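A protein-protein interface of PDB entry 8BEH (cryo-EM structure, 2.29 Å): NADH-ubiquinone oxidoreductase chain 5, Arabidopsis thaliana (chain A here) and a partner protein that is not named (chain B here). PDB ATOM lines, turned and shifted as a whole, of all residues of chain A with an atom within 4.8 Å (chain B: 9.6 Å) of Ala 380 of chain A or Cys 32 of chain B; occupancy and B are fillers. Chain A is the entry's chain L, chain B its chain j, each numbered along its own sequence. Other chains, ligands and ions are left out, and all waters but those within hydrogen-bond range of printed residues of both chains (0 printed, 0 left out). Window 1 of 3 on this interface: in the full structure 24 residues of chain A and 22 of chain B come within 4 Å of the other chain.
Along chain A the printed residues that touch a printed residue of chain B span positions 376 to 384.
Hydrophobic or aromatic side chains of chain B that line the printed part of chain A: His 24, Leu 31 and Met 35.
Along chain B the printed residues that touch a printed residue of chain A span positions 24 to 35.
Among the printed residues, 8 pairs touch across the chains.
Thr 25 of chain B touches Pro 376 of chain A.
CD2 of His 24 of chain B touches CD2 of Leu 377 of chain A, 3.7 Å away.
Leu 377 of chain A touches Thr 27 of chain B.
CA of Gly 28 of chain B touches CB of Ala 380 of chain A, 3.8 Å away.
Ala 380 of chain A touches Cys 32 of chain B.
Met 381 of chain A touches Leu 31 of chain B (CE to CD1, 3.9 Å).
Cys 32 of chain B touches Leu 383 of chain A (SG to CD2, 3.9 Å).
SD of Met 35 of chain B touches CG1 of Ile 384 of chain A (3.6 Å).
Ala 380 of chain A touches just these residues of chain B: Gly 28 and Cys 32.
Of chain A, only Ala 380 (3.7 Å) and Leu 383 (3.9 Å) come within 4 Å of Cys 32 of chain B.
Of chain B, only Leu 31 comes within 4 Å of Met 381 of chain A.
Printed residues of chain A within 4 Å of Met 35 of chain B: Ile 384 (3.6 Å).
Printed residues of chain A within 4 Å of Leu 31 of chain B: Met 381 (3.9 Å).
Of the printed residues of chain A, Thr 27 of chain B touches Leu 377.
Trp 36 of chain B touches none of the printed residues of chain A.
Ile 39 of chain B touches none of the printed residues of chain A.
The nearest residue of chain A that does not touch Cys 32 of chain B is Ile 384 of chain A (4.2 Å).
The nearest printed residue of chain A that does not touch Leu 31 of chain B is Ile 384 of chain A (4.3 Å).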
ATOM      1  N   PRO A 376     -19.831 -14.583   2.412  1.00  0.00           N
ATOM      2  CA  PRO A 376     -20.972 -15.362   2.926  1.00  0.00           C
ATOM      3  C   PRO A 376     -22.127 -15.443   1.948  1.00  0.00           C
ATOM      4  O   PRO A 376     -22.659 -16.533   1.703  1.00  0.00           O
ATOM      5  CB  PRO A 376     -21.361 -14.605   4.208  1.00  0.00           C
ATOM      6  CG  PRO A 376     -20.237 -13.669   4.482  1.00  0.00           C
ATOM      7  CD  PRO A 376     -19.625 -13.342   3.170  1.00  0.00           C
ATOM      8  N   LEU A 377     -22.531 -14.305   1.382  1.00  0.00           N
ATOM      9  CA  LEU A 377     -23.670 -14.283   0.474  1.00  0.00           C
ATOM     10  C   LEU A 377     -23.407 -15.121  -0.770  1.00  0.00           C
ATOM     11  O   LEU A 377     -24.272 -15.895  -1.205  1.00  0.00           O
ATOM     12  CB  LEU A 377     -23.998 -12.842   0.091  1.00  0.00           C
ATOM     13  CG  LEU A 377     -25.057 -12.675  -0.999  1.00  0.00           C
ATOM     14  CD1 LEU A 377     -26.373 -13.281  -0.547  1.00  0.00           C
ATOM     15  CD2 LEU A 377     -25.223 -11.213  -1.369  1.00  0.00           C
ATOM     16  N   THR A 378     -22.218 -14.985  -1.352  1.00  0.00           N
ATOM     17  CA  THR A 378     -21.899 -15.745  -2.552  1.00  0.00           C
ATOM     18  C   THR A 378     -21.831 -17.239  -2.254  1.00  0.00           C
ATOM     19  O   THR A 378     -22.332 -18.056  -3.037  1.00  0.00           O
ATOM     20  CB  THR A 378     -20.589 -15.242  -3.155  1.00  0.00           C
ATOM     21  OG1 THR A 378     -20.814 -13.985  -3.801  1.00  0.00           O
ATOM     22  CG2 THR A 378     -20.094 -16.212  -4.177  1.00  0.00           C
ATOM     23  N   TYR A 379     -21.171 -17.620  -1.166  1.00  0.00           N
ATOM     24  CA  TYR A 379     -21.179 -19.030  -0.718  1.00  0.00           C
ATOM     25  C   TYR A 379     -22.632 -19.566  -0.551  1.00  0.00           C
ATOM     26  O   TYR A 379     -22.885 -20.656  -1.008  1.00  0.00           O
ATOM     27  CB  TYR A 379     -20.424 -19.269   0.590  1.00  0.00           C
ATOM     28  CG  TYR A 379     -20.600 -20.674   1.108  1.00  0.00           C
ATOM     29  CD1 TYR A 379     -20.121 -21.752   0.385  1.00  0.00           C
ATOM     30  CD2 TYR A 379     -21.297 -20.938   2.272  1.00  0.00           C
ATOM     31  CE1 TYR A 379     -20.293 -23.051   0.813  1.00  0.00           C
ATOM     32  CE2 TYR A 379     -21.480 -22.234   2.721  1.00  0.00           C
ATOM     33  CZ  TYR A 379     -20.974 -23.291   1.990  1.00  0.00           C
ATOM     34  OH  TYR A 379     -21.153 -24.569   2.407  1.00  0.00           O
ATOM     35  N   ALA A 380     -23.502 -18.804   0.086  1.00  0.00           N
ATOM     36  CA  ALA A 380     -24.875 -19.262   0.273  1.00  0.00           C
ATOM     37  C   ALA A 380     -25.585 -19.440  -1.063  1.00  0.00           C
ATOM     38  O   ALA A 380     -26.319 -20.415  -1.259  1.00  0.00           O
ATOM     39  CB  ALA A 380     -25.643 -18.290   1.166  1.00  0.00           C
ATOM     40  N   MET A 381     -25.378 -18.505  -1.995  1.00  0.00           N
ATOM     41  CA  MET A 381     -25.981 -18.636  -3.317  1.00  0.00           C
ATOM     42  C   MET A 381     -25.479 -19.882  -4.031  1.00  0.00           C
ATOM     43  O   MET A 381     -26.265 -20.626  -4.631  1.00  0.00           O
ATOM     44  CB  MET A 381     -25.697 -17.391  -4.157  1.00  0.00           C
ATOM     45  CG  MET A 381     -26.286 -16.068  -3.660  1.00  0.00           C
ATOM     46  SD  MET A 381     -28.073 -15.940  -3.402  1.00  0.00           S
ATOM     47  CE  MET A 381     -28.312 -16.691  -1.793  1.00  0.00           C
ATOM     48  N   MET A 382     -24.170 -20.132  -3.965  1.00  0.00           N
ATOM     49  CA  MET A 382     -23.616 -21.319  -4.604  1.00  0.00           C
ATOM     50  C   MET A 382     -24.142 -22.591  -3.953  1.00  0.00           C
ATOM     51  O   MET A 382     -24.426 -23.574  -4.642  1.00  0.00           O
ATOM     52  CB  MET A 382     -22.089 -21.275  -4.569  1.00  0.00           C
ATOM     53  CG  MET A 382     -21.426 -22.192  -5.586  1.00  0.00           C
ATOM     54  SD  MET A 382     -20.821 -21.341  -7.058  1.00  0.00           S
ATOM     55  CE  MET A 382     -19.736 -20.131  -6.324  1.00  0.00           C
ATOM     56  N   LEU A 383     -24.276 -22.621  -2.641  1.00  0.00           N
ATOM     57  CA  LEU A 383     -24.870 -23.773  -1.904  1.00  0.00           C
ATOM     58  C   LEU A 383     -26.294 -24.053  -2.388  1.00  0.00           C
ATOM     59  O   LEU A 383     -26.563 -25.148  -2.766  1.00  0.00           O
ATOM     60  CB  LEU A 383     -24.855 -23.491  -0.407  1.00  0.00           C
ATOM     61  CG  LEU A 383     -25.447 -24.572   0.489  1.00  0.00           C
ATOM     62  CD1 LEU A 383     -24.684 -25.874   0.355  1.00  0.00           C
ATOM     63  CD2 LEU A 383     -25.480 -24.107   1.934  1.00  0.00           C
ATOM     64  N   ILE A 384     -27.089 -23.000  -2.420  1.00  0.00           N
ATOM     65  CA  ILE A 384     -28.484 -23.185  -2.816  1.00  0.00           C
ATOM     66  C   ILE A 384     -28.562 -23.704  -4.247  1.00  0.00           C
ATOM     67  O   ILE A 384     -29.303 -24.652  -4.544  1.00  0.00           O
ATOM     68  CB  ILE A 384     -29.267 -21.871  -2.642  1.00  0.00           C
ATOM     69  CG1 ILE A 384     -29.520 -21.590  -1.159  1.00  0.00           C
ATOM     70  CG2 ILE A 384     -30.570 -21.899  -3.431  1.00  0.00           C
ATOM     71  CD1 ILE A 384     -30.060 -20.220  -0.881  1.00  0.00           C
ATOM     72  N   HIS B  24     -24.688  -8.549   3.875  1.00  0.00           N
ATOM     73  CA  HIS B  24     -24.330  -9.736   3.107  1.00  0.00           C
ATOM     74  C   HIS B  24     -24.378 -10.985   3.979  1.00  0.00           C
ATOM     75  O   HIS B  24     -24.986 -12.000   3.605  1.00  0.00           O
ATOM     76  CB  HIS B  24     -22.946  -9.545   2.493  1.00  0.00           C
ATOM     77  CG  HIS B  24     -22.974  -8.834   1.178  1.00  0.00           C
ATOM     78  ND1 HIS B  24     -21.853  -8.653   0.403  1.00  0.00           N
ATOM     79  CD2 HIS B  24     -23.995  -8.261   0.501  1.00  0.00           C
ATOM     80  CE1 HIS B  24     -22.179  -7.998  -0.695  1.00  0.00           C
ATOM     81  NE2 HIS B  24     -23.474  -7.746  -0.660  1.00  0.00           N
ATOM     82  N   THR B  25     -23.757 -10.918   5.159  1.00  0.00           N
ATOM     83  CA  THR B  25     -23.839 -12.023   6.105  1.00  0.00           C
ATOM     84  C   THR B  25     -25.286 -12.317   6.466  1.00  0.00           C
ATOM     85  O   THR B  25     -25.709 -13.477   6.468  1.00  0.00           O
ATOM     86  CB  THR B  25     -23.031 -11.709   7.367  1.00  0.00           C
ATOM     87  OG1 THR B  25     -21.663 -11.470   7.021  1.00  0.00           O
ATOM     88  CG2 THR B  25     -23.102 -12.862   8.340  1.00  0.00           C
ATOM     89  N   VAL B  26     -26.066 -11.271   6.747  1.00  0.00           N
ATOM     90  CA  VAL B  26     -27.448 -11.464   7.179  1.00  0.00           C
ATOM     91  C   VAL B  26     -28.273 -12.104   6.070  1.00  0.00           C
ATOM     92  O   VAL B  26     -29.049 -13.034   6.313  1.00  0.00           O
ATOM     93  CB  VAL B  26     -28.058 -10.129   7.644  1.00  0.00           C
ATOM     94  CG1 VAL B  26     -29.568 -10.257   7.795  1.00  0.00           C
ATOM     95  CG2 VAL B  26     -27.429  -9.694   8.954  1.00  0.00           C
ATOM     96  N   THR B  27     -28.122 -11.616   4.837  1.00  0.00           N
ATOM     97  CA  THR B  27     -28.884 -12.159   3.720  1.00  0.00           C
ATOM     98  C   THR B  27     -28.536 -13.622   3.470  1.00  0.00           C
ATOM     99  O   THR B  27     -29.431 -14.447   3.244  1.00  0.00           O
ATOM    100  CB  THR B  27     -28.635 -11.316   2.470  1.00  0.00           C
ATOM    101  OG1 THR B  27     -29.154  -9.996   2.672  1.00  0.00           O
ATOM    102  CG2 THR B  27     -29.307 -11.926   1.265  1.00  0.00           C
ATOM    103  N   GLY B  28     -27.245 -13.968   3.513  1.00  0.00           N
ATOM    104  CA  GLY B  28     -26.870 -15.364   3.341  1.00  0.00           C
ATOM    105  C   GLY B  28     -27.420 -16.253   4.439  1.00  0.00           C
ATOM    106  O   GLY B  28     -28.035 -17.294   4.169  1.00  0.00           O
ATOM    107  N   LYS B  29     -27.121 -15.918   5.711  1.00  0.00           N
ATOM    108  CA  LYS B  29     -27.776 -16.670   6.814  1.00  0.00           C
ATOM    109  C   LYS B  29     -29.294 -16.796   6.570  1.00  0.00           C
ATOM    110  O   LYS B  29     -29.682 -17.936   6.497  1.00  0.00           O
ATOM    111  CB  LYS B  29     -27.452 -16.105   8.199  1.00  0.00           C
ATOM    112  CG  LYS B  29     -26.064 -16.417   8.732  1.00  0.00           C
ATOM    113  CD  LYS B  29     -26.019 -17.706   9.504  1.00  0.00           C
ATOM    114  CE  LYS B  29     -24.628 -18.108   9.940  1.00  0.00           C
ATOM    115  NZ  LYS B  29     -23.703 -18.212   8.789  1.00  0.00           N
ATOM    116  N   GLY B  30     -30.045 -15.717   6.313  1.00  0.00           N
ATOM    117  CA  GLY B  30     -31.491 -15.815   6.275  1.00  0.00           C
ATOM    118  C   GLY B  30     -32.015 -16.638   5.120  1.00  0.00           C
ATOM    119  O   GLY B  30     -32.951 -17.420   5.290  1.00  0.00           O
ATOM    120  N   LEU B  31     -31.441 -16.467   3.926  1.00  0.00           N
ATOM    121  CA  LEU B  31     -31.881 -17.284   2.803  1.00  0.00           C
ATOM    122  C   LEU B  31     -31.596 -18.757   3.046  1.00  0.00           C
ATOM    123  O   LEU B  31     -32.446 -19.610   2.760  1.00  0.00           O
ATOM    124  CB  LEU B  31     -31.239 -16.818   1.500  1.00  0.00           C
ATOM    125  CG  LEU B  31     -32.001 -15.708   0.785  1.00  0.00           C
ATOM    126  CD1 LEU B  31     -31.055 -14.742   0.121  1.00  0.00           C
ATOM    127  CD2 LEU B  31     -32.940 -16.314  -0.240  1.00  0.00           C
ATOM    128  N   CYS B  32     -30.428 -19.094   3.555  1.00  0.00           N
ATOM    129  CA  CYS B  32     -30.220 -20.511   3.873  1.00  0.00           C
ATOM    130  C   CYS B  32     -31.189 -20.987   4.978  1.00  0.00           C
ATOM    131  O   CYS B  32     -31.613 -22.126   4.866  1.00  0.00           O
ATOM    132  CB  CYS B  32     -28.744 -20.805   4.162  1.00  0.00           C
ATOM    133  SG  CYS B  32     -27.762 -20.965   2.644  1.00  0.00           S
ATOM    134  N   ALA B  33     -31.545 -20.144   5.939  1.00  0.00           N
ATOM    135  CA  ALA B  33     -32.422 -20.573   7.064  1.00  0.00           C
ATOM    136  C   ALA B  33     -33.785 -20.853   6.467  1.00  0.00           C
ATOM    137  O   ALA B  33     -34.319 -21.939   6.737  1.00  0.00           O
ATOM    138  CB  ALA B  33     -32.446 -19.545   8.178  1.00  0.00           C
ATOM    139  N   VAL B  34     -34.169 -19.997   5.533  1.00  0.00           N
ATOM    140  CA  VAL B  34     -35.437 -20.188   4.840  1.00  0.00           C
ATOM    141  C   VAL B  34     -35.421 -21.498   4.068  1.00  0.00           C
ATOM    142  O   VAL B  34     -36.404 -22.244   4.068  1.00  0.00           O
ATOM    143  CB  VAL B  34     -35.728 -18.986   3.920  1.00  0.00           C
ATOM    144  CG1 VAL B  34     -36.634 -19.384   2.769  1.00  0.00           C
ATOM    145  CG2 VAL B  34     -36.348 -17.856   4.704  1.00  0.00           C
ATOM    146  N   MET B  35     -34.300 -21.803   3.408  1.00  0.00           N
ATOM    147  CA  MET B  35     -34.192 -23.057   2.666  1.00  0.00           C
ATOM    148  C   MET B  35     -34.307 -24.269   3.589  1.00  0.00           C
ATOM    149  O   MET B  35     -35.017 -25.233   3.276  1.00  0.00           O
ATOM    150  CB  MET B  35     -32.874 -23.088   1.894  1.00  0.00           C
ATOM    151  CG  MET B  35     -32.430 -24.472   1.454  1.00  0.00           C
ATOM    152  SD  MET B  35     -30.825 -24.469   0.630  1.00  0.00           S
ATOM    153  CE  MET B  35     -29.743 -24.052   1.998  1.00  0.00           C
ATOM    154  N   TRP B  36     -33.636 -24.273   4.714  1.00  0.00           N
ATOM    155  CA  TRP B  36     -33.669 -25.388   5.713  1.00  0.00           C
ATOM    156  C   TRP B  36     -35.086 -25.546   6.280  1.00  0.00           C
ATOM    157  O   TRP B  36     -35.557 -26.677   6.314  1.00  0.00           O
ATOM    158  CB  TRP B  36     -32.622 -25.210   6.815  1.00  0.00           C
ATOM    159  CG  TRP B  36     -31.202 -25.095   6.355  1.00  0.00           C
ATOM    160  CD1 TRP B  36     -30.340 -24.073   6.612  1.00  0.00           C
ATOM    161  CD2 TRP B  36     -30.469 -26.046   5.565  1.00  0.00           C
ATOM    162  NE1 TRP B  36     -29.130 -24.310   6.032  1.00  0.00           N
ATOM    163  CE2 TRP B  36     -29.175 -25.516   5.386  1.00  0.00           C
ATOM    164  CE3 TRP B  36     -30.771 -27.280   4.992  1.00  0.00           C
ATOM    165  CZ2 TRP B  36     -28.190 -26.191   4.667  1.00  0.00           C
ATOM    166  CZ3 TRP B  36     -29.807 -27.944   4.269  1.00  0.00           C
ATOM    167  CH2 TRP B  36     -28.528 -27.402   4.112  1.00  0.00           C
ATOM    168  N   PHE B  37     -35.733 -24.437   6.596  1.00  0.00           N
ATOM    169  CA  PHE B  37     -37.102 -24.511   7.094  1.00  0.00           C
ATOM    170  C   PHE B  37     -38.045 -25.047   6.029  1.00  0.00           C
ATOM    171  O   PHE B  37     -38.934 -25.853   6.325  1.00  0.00           O
ATOM    172  CB  PHE B  37     -37.574 -23.137   7.569  1.00  0.00           C
ATOM    173  CG  PHE B  37     -39.003 -23.118   8.044  1.00  0.00           C
ATOM    174  CD1 PHE B  37     -40.038 -22.812   7.176  1.00  0.00           C
ATOM    175  CD2 PHE B  37     -39.310 -23.409   9.365  1.00  0.00           C
ATOM    176  CE1 PHE B  37     -41.344 -22.798   7.609  1.00  0.00           C
ATOM    177  CE2 PHE B  37     -40.614 -23.394   9.803  1.00  0.00           C
ATOM    178  CZ  PHE B  37     -41.634 -23.088   8.925  1.00  0.00           C
ATOM    179  N   TRP B  38     -37.878 -24.597   4.785  1.00  0.00           N
ATOM    180  CA  TRP B  38     -38.722 -25.073   3.699  1.00  0.00           C
ATOM    181  C   TRP B  38     -38.549 -26.570   3.490  1.00  0.00           C
ATOM    182  O   TRP B  38     -39.530 -27.292   3.281  1.00  0.00           O
ATOM    183  CB  TRP B  38     -38.393 -24.295   2.426  1.00  0.00           C
ATOM    184  CG  TRP B  38     -38.972 -24.850   1.174  1.00  0.00           C
ATOM    185  CD1 TRP B  38     -38.318 -25.568   0.224  1.00  0.00           C
ATOM    186  CD2 TRP B  38     -40.321 -24.718   0.721  1.00  0.00           C
ATOM    187  NE1 TRP B  38     -39.174 -25.895  -0.797  1.00  0.00           N
ATOM    188  CE2 TRP B  38     -40.412 -25.386  -0.514  1.00  0.00           C
ATOM    189  CE3 TRP B  38     -41.464 -24.109   1.244  1.00  0.00           C
ATOM    190  CZ2 TRP B  38     -41.600 -25.457  -1.236  1.00  0.00           C
ATOM    191  CZ3 TRP B  38     -42.639 -24.179   0.523  1.00  0.00           C
ATOM    192  CH2 TRP B  38     -42.699 -24.850  -0.702  1.00  0.00           C
ATOM    193  N   ILE B  39     -37.310 -27.055   3.563  1.00  0.00           N
ATOM    194  CA  ILE B  39     -37.071 -28.487   3.420  1.00  0.00           C
ATOM    195  C   ILE B  39     -37.750 -29.258   4.546  1.00  0.00           C
ATOM    196  O   ILE B  39     -38.386 -30.289   4.311  1.00  0.00           O
ATOM    197  CB  ILE B  39     -35.561 -28.774   3.360  1.00  0.00           C
ATOM    198  CG1 ILE B  39     -34.980 -28.280   2.034  1.00  0.00           C
ATOM    199  CG2 ILE B  39     -35.284 -30.264   3.544  1.00  0.00           C
ATOM    200  CD1 ILE B  39     -33.475 -28.254   2.005  1.00  0.00           C
ATOM    201  N   LEU B  40     -37.629 -28.772   5.785  1.00  0.00           N
ATOM    202  CA  LEU B  40     -38.246 -29.471   6.913  1.00  0.00           C
ATOM    203  C   LEU B  40     -39.766 -29.497   6.790  1.00  0.00           C
ATOM    204  O   LEU B  40     -40.400 -30.541   6.995  1.00  0.00           O
ATOM    205  CB  LEU B  40     -37.824 -28.813   8.224  1.00  0.00           C
ATOM    206  CG  LEU B  40     -36.360 -29.008   8.608  1.00  0.00           C
ATOM    207  CD1 LEU B  40     -36.035 -28.256   9.883  1.00  0.00           C
ATOM    208  CD2 LEU B  40     -36.022 -30.485   8.744  1.00  0.00           C
